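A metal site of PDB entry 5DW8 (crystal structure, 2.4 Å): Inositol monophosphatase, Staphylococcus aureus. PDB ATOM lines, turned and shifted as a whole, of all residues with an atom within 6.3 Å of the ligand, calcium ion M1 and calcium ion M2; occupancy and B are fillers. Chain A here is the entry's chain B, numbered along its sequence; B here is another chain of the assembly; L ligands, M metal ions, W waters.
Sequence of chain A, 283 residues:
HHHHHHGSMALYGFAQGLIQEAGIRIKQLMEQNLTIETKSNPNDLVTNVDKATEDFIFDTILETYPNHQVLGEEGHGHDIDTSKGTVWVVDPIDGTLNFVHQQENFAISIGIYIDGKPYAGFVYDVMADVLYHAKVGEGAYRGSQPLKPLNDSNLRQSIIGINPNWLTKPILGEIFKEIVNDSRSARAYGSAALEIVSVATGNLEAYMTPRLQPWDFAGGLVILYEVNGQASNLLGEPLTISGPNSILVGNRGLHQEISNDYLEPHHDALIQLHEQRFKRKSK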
ATOM      1  N   ASP A  50      -6.907 -21.987 -10.388  1.00  0.00           N
ATOM      2  CA  ASP A  50      -7.276 -20.573 -10.413  1.00  0.00           C
ATOM      3  C   ASP A  50      -8.747 -20.327 -10.728  1.00  0.00           C
ATOM      4  O   ASP A  50      -9.348 -19.414 -10.173  1.00  0.00           O
ATOM      5  CB  ASP A  50      -6.397 -19.809 -11.413  1.00  0.00           C
ATOM      6  CG  ASP A  50      -6.782 -18.372 -11.510  1.00  0.00           C
ATOM      7  OD1 ASP A  50      -7.728 -18.025 -12.273  1.00  0.00           O
ATOM      8  OD2 ASP A  50      -6.148 -17.581 -10.799  1.00  0.00           O
ATOM      9  N   GLU A  73     -10.326 -10.417 -12.503  1.00  0.00           N
ATOM     10  CA  GLU A  73      -9.604 -10.699 -13.739  1.00  0.00           C
ATOM     11  C   GLU A  73     -10.508 -11.127 -14.888  1.00  0.00           C
ATOM     12  O   GLU A  73     -11.631 -11.600 -14.682  1.00  0.00           O
ATOM     13  CB  GLU A  73      -8.577 -11.805 -13.477  1.00  0.00           C
ATOM     14  CG  GLU A  73      -7.562 -11.443 -12.413  1.00  0.00           C
ATOM     15  CD  GLU A  73      -6.635 -12.590 -12.095  1.00  0.00           C
ATOM     16  OE1 GLU A  73      -7.131 -13.659 -11.666  1.00  0.00           O
ATOM     17  OE2 GLU A  73      -5.414 -12.414 -12.272  1.00  0.00           O
ATOM     18  N   ASP A  91      -8.308 -10.650  -6.595  1.00  0.00           N
ATOM     19  CA  ASP A  91      -7.370 -11.420  -7.399  1.00  0.00           C
ATOM     20  C   ASP A  91      -7.224 -12.799  -6.730  1.00  0.00           C
ATOM     21  O   ASP A  91      -6.694 -12.892  -5.635  1.00  0.00           O
ATOM     22  CB  ASP A  91      -6.012 -10.705  -7.478  1.00  0.00           C
ATOM     23  CG  ASP A  91      -5.018 -11.397  -8.391  1.00  0.00           C
ATOM     24  OD1 ASP A  91      -5.239 -12.544  -8.864  1.00  0.00           O
ATOM     25  OD2 ASP A  91      -3.963 -10.759  -8.619  1.00  0.00           O
ATOM     26  N   PRO A  92      -7.708 -13.861  -7.378  1.00  0.00           N
ATOM     27  CA  PRO A  92      -7.748 -15.160  -6.692  1.00  0.00           C
ATOM     28  C   PRO A  92      -6.412 -15.794  -6.489  1.00  0.00           C
ATOM     29  O   PRO A  92      -6.230 -16.510  -5.495  1.00  0.00           O
ATOM     30  CB  PRO A  92      -8.588 -16.045  -7.618  1.00  0.00           C
ATOM     31  CG  PRO A  92      -8.685 -15.328  -8.916  1.00  0.00           C
ATOM     32  CD  PRO A  92      -8.566 -13.867  -8.579  1.00  0.00           C
ATOM     33  N   ILE A  93      -5.484 -15.605  -7.415  1.00  0.00           N
ATOM     34  CA  ILE A  93      -4.082 -15.977  -7.175  1.00  0.00           C
ATOM     35  C   ILE A  93      -3.249 -14.827  -7.681  1.00  0.00           C
ATOM     36  O   ILE A  93      -3.189 -14.614  -8.900  1.00  0.00           O
ATOM     37  CB  ILE A  93      -3.654 -17.238  -7.957  1.00  0.00           C
ATOM     38  CG1 ILE A  93      -4.383 -18.472  -7.440  1.00  0.00           C
ATOM     39  CG2 ILE A  93      -2.142 -17.467  -7.866  1.00  0.00           C
ATOM     40  CD1 ILE A  93      -4.314 -19.645  -8.405  1.00  0.00           C
ATOM     41  N   ASP A  94      -2.643 -14.079  -6.756  1.00  0.00           N
ATOM     42  CA  ASP A  94      -1.632 -13.119  -7.124  1.00  0.00           C
ATOM     43  C   ASP A  94      -0.228 -13.679  -6.956  1.00  0.00           C
ATOM     44  O   ASP A  94       0.201 -14.053  -5.855  1.00  0.00           O
ATOM     45  CB  ASP A  94      -1.755 -11.873  -6.279  1.00  0.00           C
ATOM     46  CG  ASP A  94      -0.783 -10.793  -6.729  1.00  0.00           C
ATOM     47  OD1 ASP A  94      -0.948 -10.268  -7.843  1.00  0.00           O
ATOM     48  OD2 ASP A  94       0.130 -10.428  -5.950  1.00  0.00           O
ATOM     49  N   GLY A  95       0.505 -13.653  -8.055  1.00  0.00           N
ATOM     50  CA  GLY A  95       1.766 -14.356  -8.179  1.00  0.00           C
ATOM     51  C   GLY A  95       1.527 -15.729  -8.791  1.00  0.00           C
ATOM     52  O   GLY A  95       2.012 -16.734  -8.256  1.00  0.00           O
ATOM     53  N   THR A  96       0.796 -15.776  -9.905  1.00  0.00           N
ATOM     54  CA  THR A  96       0.550 -17.029 -10.594  1.00  0.00           C
ATOM     55  C   THR A  96       1.858 -17.717 -11.012  1.00  0.00           C
ATOM     56  O   THR A  96       1.952 -18.937 -10.893  1.00  0.00           O
ATOM     57  CB  THR A  96      -0.427 -16.910 -11.817  1.00  0.00           C
ATOM     58  OG1 THR A  96      -0.100 -15.787 -12.635  1.00  0.00           O
ATOM     59  CG2 THR A  96      -1.851 -16.752 -11.325  1.00  0.00           C
ATOM     60  N   LEU A  97       2.838 -16.954 -11.487  1.00  0.00           N
ATOM     61  CA  LEU A  97       4.132 -17.534 -11.840  1.00  0.00           C
ATOM     62  C   LEU A  97       4.816 -18.181 -10.645  1.00  0.00           C
ATOM     63  O   LEU A  97       5.364 -19.240 -10.760  1.00  0.00           O
ATOM     64  CB  LEU A  97       5.061 -16.516 -12.459  1.00  0.00           C
ATOM     65  CG  LEU A  97       4.760 -16.099 -13.887  1.00  0.00           C
ATOM     66  CD1 LEU A  97       5.567 -14.851 -14.259  1.00  0.00           C
ATOM     67  CD2 LEU A  97       5.082 -17.234 -14.827  1.00  0.00           C
ATOM     68  N   ASN A 163      11.139  -4.617  -9.882  1.00  0.00           N
ATOM     69  CA  ASN A 163      11.490  -5.735 -10.705  1.00  0.00           C
ATOM     70  C   ASN A 163      12.551  -5.379 -11.788  1.00  0.00           C
ATOM     71  O   ASN A 163      12.507  -4.302 -12.377  1.00  0.00           O
ATOM     72  CB  ASN A 163      10.243  -6.331 -11.336  1.00  0.00           C
ATOM     73  CG  ASN A 163      10.493  -7.737 -11.836  1.00  0.00           C
ATOM     74  OD1 ASN A 163      10.178  -8.710 -11.152  1.00  0.00           O
ATOM     75  ND2 ASN A 163      11.088  -7.846 -13.015  1.00  0.00           N
ATOM     76  N   GLY A 190       7.779 -10.944  -7.201  1.00  0.00           N
ATOM     77  CA  GLY A 190       6.816 -11.604  -8.106  1.00  0.00           C
ATOM     78  C   GLY A 190       5.364 -11.616  -7.644  1.00  0.00           C
ATOM     79  O   GLY A 190       4.501 -12.172  -8.321  1.00  0.00           O
ATOM     80  N   SER A 191       5.090 -11.001  -6.487  1.00  0.00           N
ATOM     81  CA  SER A 191       3.723 -10.726  -6.069  1.00  0.00           C
ATOM     82  C   SER A 191       3.584  -9.290  -5.669  1.00  0.00           C
ATOM     83  O   SER A 191       4.254  -8.847  -4.752  1.00  0.00           O
ATOM     84  CB  SER A 191       3.313 -11.573  -4.860  1.00  0.00           C
ATOM     85  OG  SER A 191       2.036 -11.165  -4.436  1.00  0.00           O
ATOM     86  N   ALA A 192       2.659  -8.589  -6.302  1.00  0.00           N
ATOM     87  CA  ALA A 192       2.336  -7.221  -5.885  1.00  0.00           C
ATOM     88  C   ALA A 192       1.666  -7.156  -4.471  1.00  0.00           C
ATOM     89  O   ALA A 192       2.023  -6.318  -3.632  1.00  0.00           O
ATOM     90  CB  ALA A 192       1.439  -6.546  -6.916  1.00  0.00           C
ATOM     91  N   ALA A 193       0.708  -8.024  -4.233  1.00  0.00           N
ATOM     92  CA  ALA A 193      -0.021  -7.999  -2.951  1.00  0.00           C
ATOM     93  C   ALA A 193       0.876  -8.282  -1.752  1.00  0.00           C
ATOM     94  O   ALA A 193       0.722  -7.717  -0.705  1.00  0.00           O
ATOM     95  CB  ALA A 193      -1.210  -8.983  -2.993  1.00  0.00           C
ATOM     96  N   GLU A 195       4.203  -7.798  -1.845  1.00  0.00           N
ATOM     97  CA  GLU A 195       5.147  -6.678  -1.823  1.00  0.00           C
ATOM     98  C   GLU A 195       4.588  -5.371  -1.288  1.00  0.00           C
ATOM     99  O   GLU A 195       5.316  -4.605  -0.637  1.00  0.00           O
ATOM    100  CB  GLU A 195       5.721  -6.448  -3.193  1.00  0.00           C
ATOM    101  CG  GLU A 195       6.748  -7.498  -3.459  1.00  0.00           C
ATOM    102  CD  GLU A 195       7.242  -7.457  -4.850  1.00  0.00           C
ATOM    103  OE1 GLU A 195       6.526  -7.876  -5.750  1.00  0.00           O
ATOM    104  OE2 GLU A 195       8.357  -6.996  -5.023  1.00  0.00           O
ATOM    105  N   TYR A 207       7.890   0.173  -2.612  1.00  0.00           N
ATOM    106  CA  TYR A 207       7.691  -0.696  -3.749  1.00  0.00           C
ATOM    107  C   TYR A 207       7.054   0.091  -4.923  1.00  0.00           C
ATOM    108  O   TYR A 207       6.113   0.890  -4.739  1.00  0.00           O
ATOM    109  CB  TYR A 207       6.830  -1.879  -3.326  1.00  0.00           C
ATOM    110  CG  TYR A 207       6.154  -2.632  -4.451  1.00  0.00           C
ATOM    111  CD1 TYR A 207       6.885  -3.443  -5.324  1.00  0.00           C
ATOM    112  CD2 TYR A 207       4.791  -2.558  -4.615  1.00  0.00           C
ATOM    113  CE1 TYR A 207       6.270  -4.159  -6.340  1.00  0.00           C
ATOM    114  CE2 TYR A 207       4.154  -3.274  -5.627  1.00  0.00           C
ATOM    115  CZ  TYR A 207       4.894  -4.080  -6.468  1.00  0.00           C
ATOM    116  OH  TYR A 207       4.238  -4.760  -7.463  1.00  0.00           O
ATOM    117  N   THR A 209       6.190   0.039  -9.473  1.00  0.00           N
ATOM    118  CA  THR A 209       5.921  -0.657 -10.697  1.00  0.00           C
ATOM    119  C   THR A 209       5.054   0.282 -11.530  1.00  0.00           C
ATOM    120  O   THR A 209       4.230   1.059 -10.967  1.00  0.00           O
ATOM    121  CB  THR A 209       5.171  -1.950 -10.439  1.00  0.00           C
ATOM    122  OG1 THR A 209       4.761  -2.498 -11.684  1.00  0.00           O
ATOM    123  CG2 THR A 209       3.939  -1.670  -9.483  1.00  0.00           C
ATOM    124  N   ARG A 211       2.854  -0.487 -13.910  1.00  0.00           N
ATOM    125  CA  ARG A 211       1.503  -1.024 -14.222  1.00  0.00           C
ATOM    126  C   ARG A 211       0.987  -2.054 -13.190  1.00  0.00           C
ATOM    127  O   ARG A 211       1.731  -2.924 -12.692  1.00  0.00           O
ATOM    128  CB  ARG A 211       1.435  -1.628 -15.638  1.00  0.00           C
ATOM    129  CG  ARG A 211       2.606  -2.529 -16.039  1.00  0.00           C
ATOM    130  CD  ARG A 211       2.351  -4.021 -15.910  1.00  0.00           C
ATOM    131  NE  ARG A 211       2.723  -4.528 -14.593  1.00  0.00           N
ATOM    132  CZ  ARG A 211       3.389  -5.661 -14.344  1.00  0.00           C
ATOM    133  NH1 ARG A 211       3.820  -6.456 -15.330  1.00  0.00           N
ATOM    134  NH2 ARG A 211       3.661  -5.982 -13.080  1.00  0.00           N
ATOM    135  N   LEU A 212      -0.295  -1.933 -12.868  1.00  0.00           N
ATOM    136  CA  LEU A 212      -0.926  -2.844 -11.916  1.00  0.00           C
ATOM    137  C   LEU A 212      -2.472  -2.718 -12.007  1.00  0.00           C
ATOM    138  O   LEU A 212      -2.976  -1.631 -12.207  1.00  0.00           O
ATOM    139  CB  LEU A 212      -0.388  -2.498 -10.527  1.00  0.00           C
ATOM    140  CG  LEU A 212      -0.082  -3.609  -9.530  1.00  0.00           C
ATOM    141  CD1 LEU A 212       0.868  -4.674 -10.087  1.00  0.00           C
ATOM    142  CD2 LEU A 212       0.485  -3.018  -8.245  1.00  0.00           C
ATOM    143  N   GLN A 213      -3.208  -3.823 -11.848  1.00  0.00           N
ATOM    144  CA  GLN A 213      -4.688  -3.789 -11.892  1.00  0.00           C
ATOM    145  C   GLN A 213      -5.279  -3.520 -10.491  1.00  0.00           C
ATOM    146  O   GLN A 213      -4.589  -3.748  -9.506  1.00  0.00           O
ATOM    147  CB  GLN A 213      -5.256  -5.097 -12.439  1.00  0.00           C
ATOM    148  CG  GLN A 213      -4.902  -5.397 -13.898  1.00  0.00           C
ATOM    149  CD  GLN A 213      -5.476  -4.387 -14.853  1.00  0.00           C
ATOM    150  OE1 GLN A 213      -6.543  -3.790 -14.612  1.00  0.00           O
ATOM    151  NE2 GLN A 213      -4.767  -4.157 -15.911  1.00  0.00           N
ATOM    152  N   TRP A 215      -7.412  -5.108  -8.724  1.00  0.00           N
ATOM    153  CA  TRP A 215      -7.308  -6.351  -7.918  1.00  0.00           C
ATOM    154  C   TRP A 215      -5.895  -6.742  -7.440  1.00  0.00           C
ATOM    155  O   TRP A 215      -5.756  -7.650  -6.628  1.00  0.00           O
ATOM    156  CB  TRP A 215      -7.969  -7.554  -8.624  1.00  0.00           C
ATOM    157  CG  TRP A 215      -7.603  -7.714 -10.031  1.00  0.00           C
ATOM    158  CD1 TRP A 215      -6.596  -8.453 -10.506  1.00  0.00           C
ATOM    159  CD2 TRP A 215      -8.237  -7.110 -11.159  1.00  0.00           C
ATOM    160  NE1 TRP A 215      -6.544  -8.363 -11.861  1.00  0.00           N
ATOM    161  CE2 TRP A 215      -7.528  -7.526 -12.294  1.00  0.00           C
ATOM    162  CE3 TRP A 215      -9.324  -6.246 -11.315  1.00  0.00           C
ATOM    163  CZ2 TRP A 215      -7.880  -7.119 -13.588  1.00  0.00           C
ATOM    164  CZ3 TRP A 215      -9.654  -5.839 -12.612  1.00  0.00           C
ATOM    165  CH2 TRP A 215      -8.946  -6.300 -13.718  1.00  0.00           C
ATOM    166  N   ASP A 216      -4.853  -6.070  -7.940  1.00  0.00           N
ATOM    167  CA  ASP A 216      -3.477  -6.321  -7.462  1.00  0.00           C
ATOM    168  C   ASP A 216      -3.209  -5.585  -6.167  1.00  0.00           C
ATOM    169  O   ASP A 216      -2.486  -6.067  -5.302  1.00  0.00           O
ATOM    170  CB  ASP A 216      -2.460  -5.882  -8.517  1.00  0.00           C
ATOM    171  CG  ASP A 216      -2.472  -6.750  -9.760  1.00  0.00           C
ATOM    172  OD1 ASP A 216      -2.476  -6.177 -10.862  1.00  0.00           O
ATOM    173  OD2 ASP A 216      -2.451  -8.011  -9.638  1.00  0.00           O
ATOM    174  N   SER B 185      10.511 -14.202 -16.134  1.00  0.00           N
ATOM    175  CA  SER B 185      10.467 -13.136 -15.115  1.00  0.00           C
ATOM    176  C   SER B 185      11.676 -13.163 -14.173  1.00  0.00           C
ATOM    177  O   SER B 185      12.410 -14.150 -14.080  1.00  0.00           O
ATOM    178  CB  SER B 185       9.181 -13.212 -14.281  1.00  0.00           C
ATOM    179  OG  SER B 185       9.020 -12.041 -13.491  1.00  0.00           O
ATOM    180  N   ARG B 187      13.552 -12.036 -10.270  1.00  0.00           N
ATOM    181  CA  ARG B 187      13.446 -11.976  -8.822  1.00  0.00           C
ATOM    182  C   ARG B 187      14.806 -11.513  -8.258  1.00  0.00           C
ATOM    183  O   ARG B 187      15.862 -11.620  -8.897  1.00  0.00           O
ATOM    184  CB  ARG B 187      13.189 -13.367  -8.229  1.00  0.00           C
ATOM    185  CG  ARG B 187      11.958 -14.095  -8.717  1.00  0.00           C
ATOM    186  CD  ARG B 187      10.703 -13.375  -8.256  1.00  0.00           C
ATOM    187  NE  ARG B 187       9.449 -13.975  -8.715  1.00  0.00           N
ATOM    188  CZ  ARG B 187       8.826 -13.702  -9.849  1.00  0.00           C
ATOM    189  NH1 ARG B 187       9.361 -12.874 -10.743  1.00  0.00           N
ATOM    190  NH2 ARG B 187       7.671 -14.282 -10.121  1.00  0.00           N
HETATM  191  P1  LIG L   1      -0.634 -12.147 -11.405  1.00  0.00           P
HETATM  192  O1  LIG L   1      -0.382 -12.407 -12.991  1.00  0.00           O
HETATM  193  O2  LIG L   1      -1.998 -12.573 -10.993  1.00  0.00           O
HETATM  194  O3  LIG L   1       0.511 -13.030 -10.706  1.00  0.00           O
HETATM  195  C1  LIG L   1       4.231  -8.992 -10.801  1.00  0.00           C
HETATM  196  O4  LIG L   1       4.014  -9.744 -12.010  1.00  0.00           O
HETATM  197  C2  LIG L   1       2.831  -8.618 -10.272  1.00  0.00           C
HETATM  198  O5  LIG L   1       2.036  -7.788 -11.204  1.00  0.00           O
HETATM  199  C3  LIG L   1       1.980  -9.832  -9.975  1.00  0.00           C
HETATM  200  O6  LIG L   1       1.260  -9.511  -8.812  1.00  0.00           O
HETATM  201  C4  LIG L   1       1.080  -9.976 -11.247  1.00  0.00           C
HETATM  202  O7  LIG L   1      -0.256 -10.562 -11.050  1.00  0.00           O
HETATM  203  C5  LIG L   1       0.959  -8.539 -11.801  1.00  0.00           C
HETATM  204  N1  LIG L   1       1.051  -8.498 -13.324  1.00  0.00           N
HETATM  205  C6  LIG L   1       1.686  -9.346 -14.167  1.00  0.00           C
HETATM  206  N2  LIG L   1       1.485  -8.932 -15.420  1.00  0.00           N
HETATM  207  C7  LIG L   1       0.725  -7.820 -15.361  1.00  0.00           C
HETATM  208  C8  LIG L   1       0.245  -7.003 -16.330  1.00  0.00           C
HETATM  209  N3  LIG L   1       0.559  -7.347 -17.585  1.00  0.00           N
HETATM  210  N4  LIG L   1      -0.505  -5.899 -16.075  1.00  0.00           N
HETATM  211  C9  LIG L   1      -0.789  -5.617 -14.738  1.00  0.00           C
HETATM  212  N5  LIG L   1      -0.281  -6.487 -13.729  1.00  0.00           N
HETATM  213  C10 LIG L   1       0.458  -7.560 -14.061  1.00  0.00           C
HETATM  214 CA    CA M   1      -3.771 -13.430 -10.772  1.00  0.00          CA
HETATM  215 CA    CA M   2      -2.390 -10.185  -9.837  1.00  0.00          CA
HETATM  216  O   HOH W   1      -2.421  -8.054 -12.575  1.00  0.00           O
HETATM  217  O   HOH W   2      -5.142 -14.944 -10.404  1.00  0.00           O
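CG2 of Thr 96 touches calcium ion M1 (3.9 Å).
Of the 24 residues printed, 4 come within 4 Å of calcium ion M1.
The nearest printed residue that does not touch calcium ion M1 is Asp 94 (4.2 Å).
Gly 190 touches the ligand.
Ser 191 touches the ligand.
Leu 212 touches the ligand.
Hydrophobic or aromatic side chains that line the ligand: Ala 192 and Leu 212.
Within 4 Å of the ligand: Glu 73, Asp 91, Ile 93, Asp 94, Gly 95, Thr 96, Gly 190, Ser 191, Ala 192, Arg 211, Leu 212 and Asp 216.
Along chain A the residues within 4 Å of the ligand span positions 73 to 216.
The nearest printed residue that does not touch the ligand is Gln 213 (4.2 Å).
Water W2 lies within hydrogen-bond range of the side-chain carboxylate (OE1) of Glu 73 (2.7 Å), the side-chain carboxylate (OD2) of Asp 50 (2.8 Å) and the backbone NH (N) of Ile 93 (3.1 Å).
Water W1 lies within hydrogen-bond range of the side-chain carboxylate of Asp 216 (2.5 Å) and a nitrogen (N5) of the ligand (2.9 Å).
Of the 24 residues printed, 3 come within 4 Å of calcium ion M2.
Along chain A the residues within 4 Å of calcium ion M2 span positions 91 to 216.
The backbone NH (N) of Thr 96 sits at hydrogen-bond distance from an oxygen (O3) of the ligand (2.9 Å).
The side-chain hydroxyl of Thr 96 sits at hydrogen-bond distance from an oxygen (O1) of the ligand.
An oxygen (O3) of the ligand is in hydrogen-bond range of the backbone NH of Gly 95, 2.7 Å away.
O5 of the ligand sits at hydrogen-bond distance from NH2 of Arg 211.
An oxygen (O6) of the ligand lies within hydrogen-bond range of the backbone NH (N) of Ala 192, at 3.0 Å.
Calcium ion M1 is bound by an oxygen (O2) of the ligand (2.0 Å), water W2 (2.1 Å), the backbone carbonyl oxygen (O) of Ile 93 (2.3 Å), the side-chain carboxylate (OE2) of Glu 73 (2.4 Å) and the side-chain carboxylate (OD1) of Asp 91 (2.6 Å).
Calcium ion M1 has five donor atoms within binding distance.
The backbone carbonyl oxygen (O) of Arg 211 sits at hydrogen-bond distance from the side-chain hydroxyl (OG1) of Thr 209 (3.2 Å).
The side-chain carboxylate (OD2) of Asp 94 lies within hydrogen-bond range of the backbone NH (N) of Ala 193.
The backbone NH of Ala 192 lies within hydrogen-bond range of the side-chain carboxylate of Asp 94.
The side-chain carboxylate of Glu 195 sits close to the backbone carbonyl oxygen of Ser 191 (2.7 Å).
The side-chain hydroxyl (OG) of Ser 191 is in hydrogen-bond range of the backbone NH (N) of Ala 193, at 3.4 Å.
The side-chain carboxylate of Asp 216 lies within hydrogen-bond range of the backbone NH of Gln 213 (2.7 Å).
The side-chain carboxylate (OD2) of Asp 94 is in hydrogen-bond range of the side-chain hydroxyl (OG) of Ser 191, 2.5 Å away.
Calcium ion M2 is bound by OD2 of Asp 91, 2.1 Å away.
OD2 of Asp 216 is bound to calcium ion M2 (2.2 Å).
OD1 of Asp 94 is bound to calcium ion M2 (2.5 Å).
An oxygen (O7) of the ligand binds calcium ion M2.
An oxygen (O2) of the ligand binds calcium ion M2 (2.7 Å).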
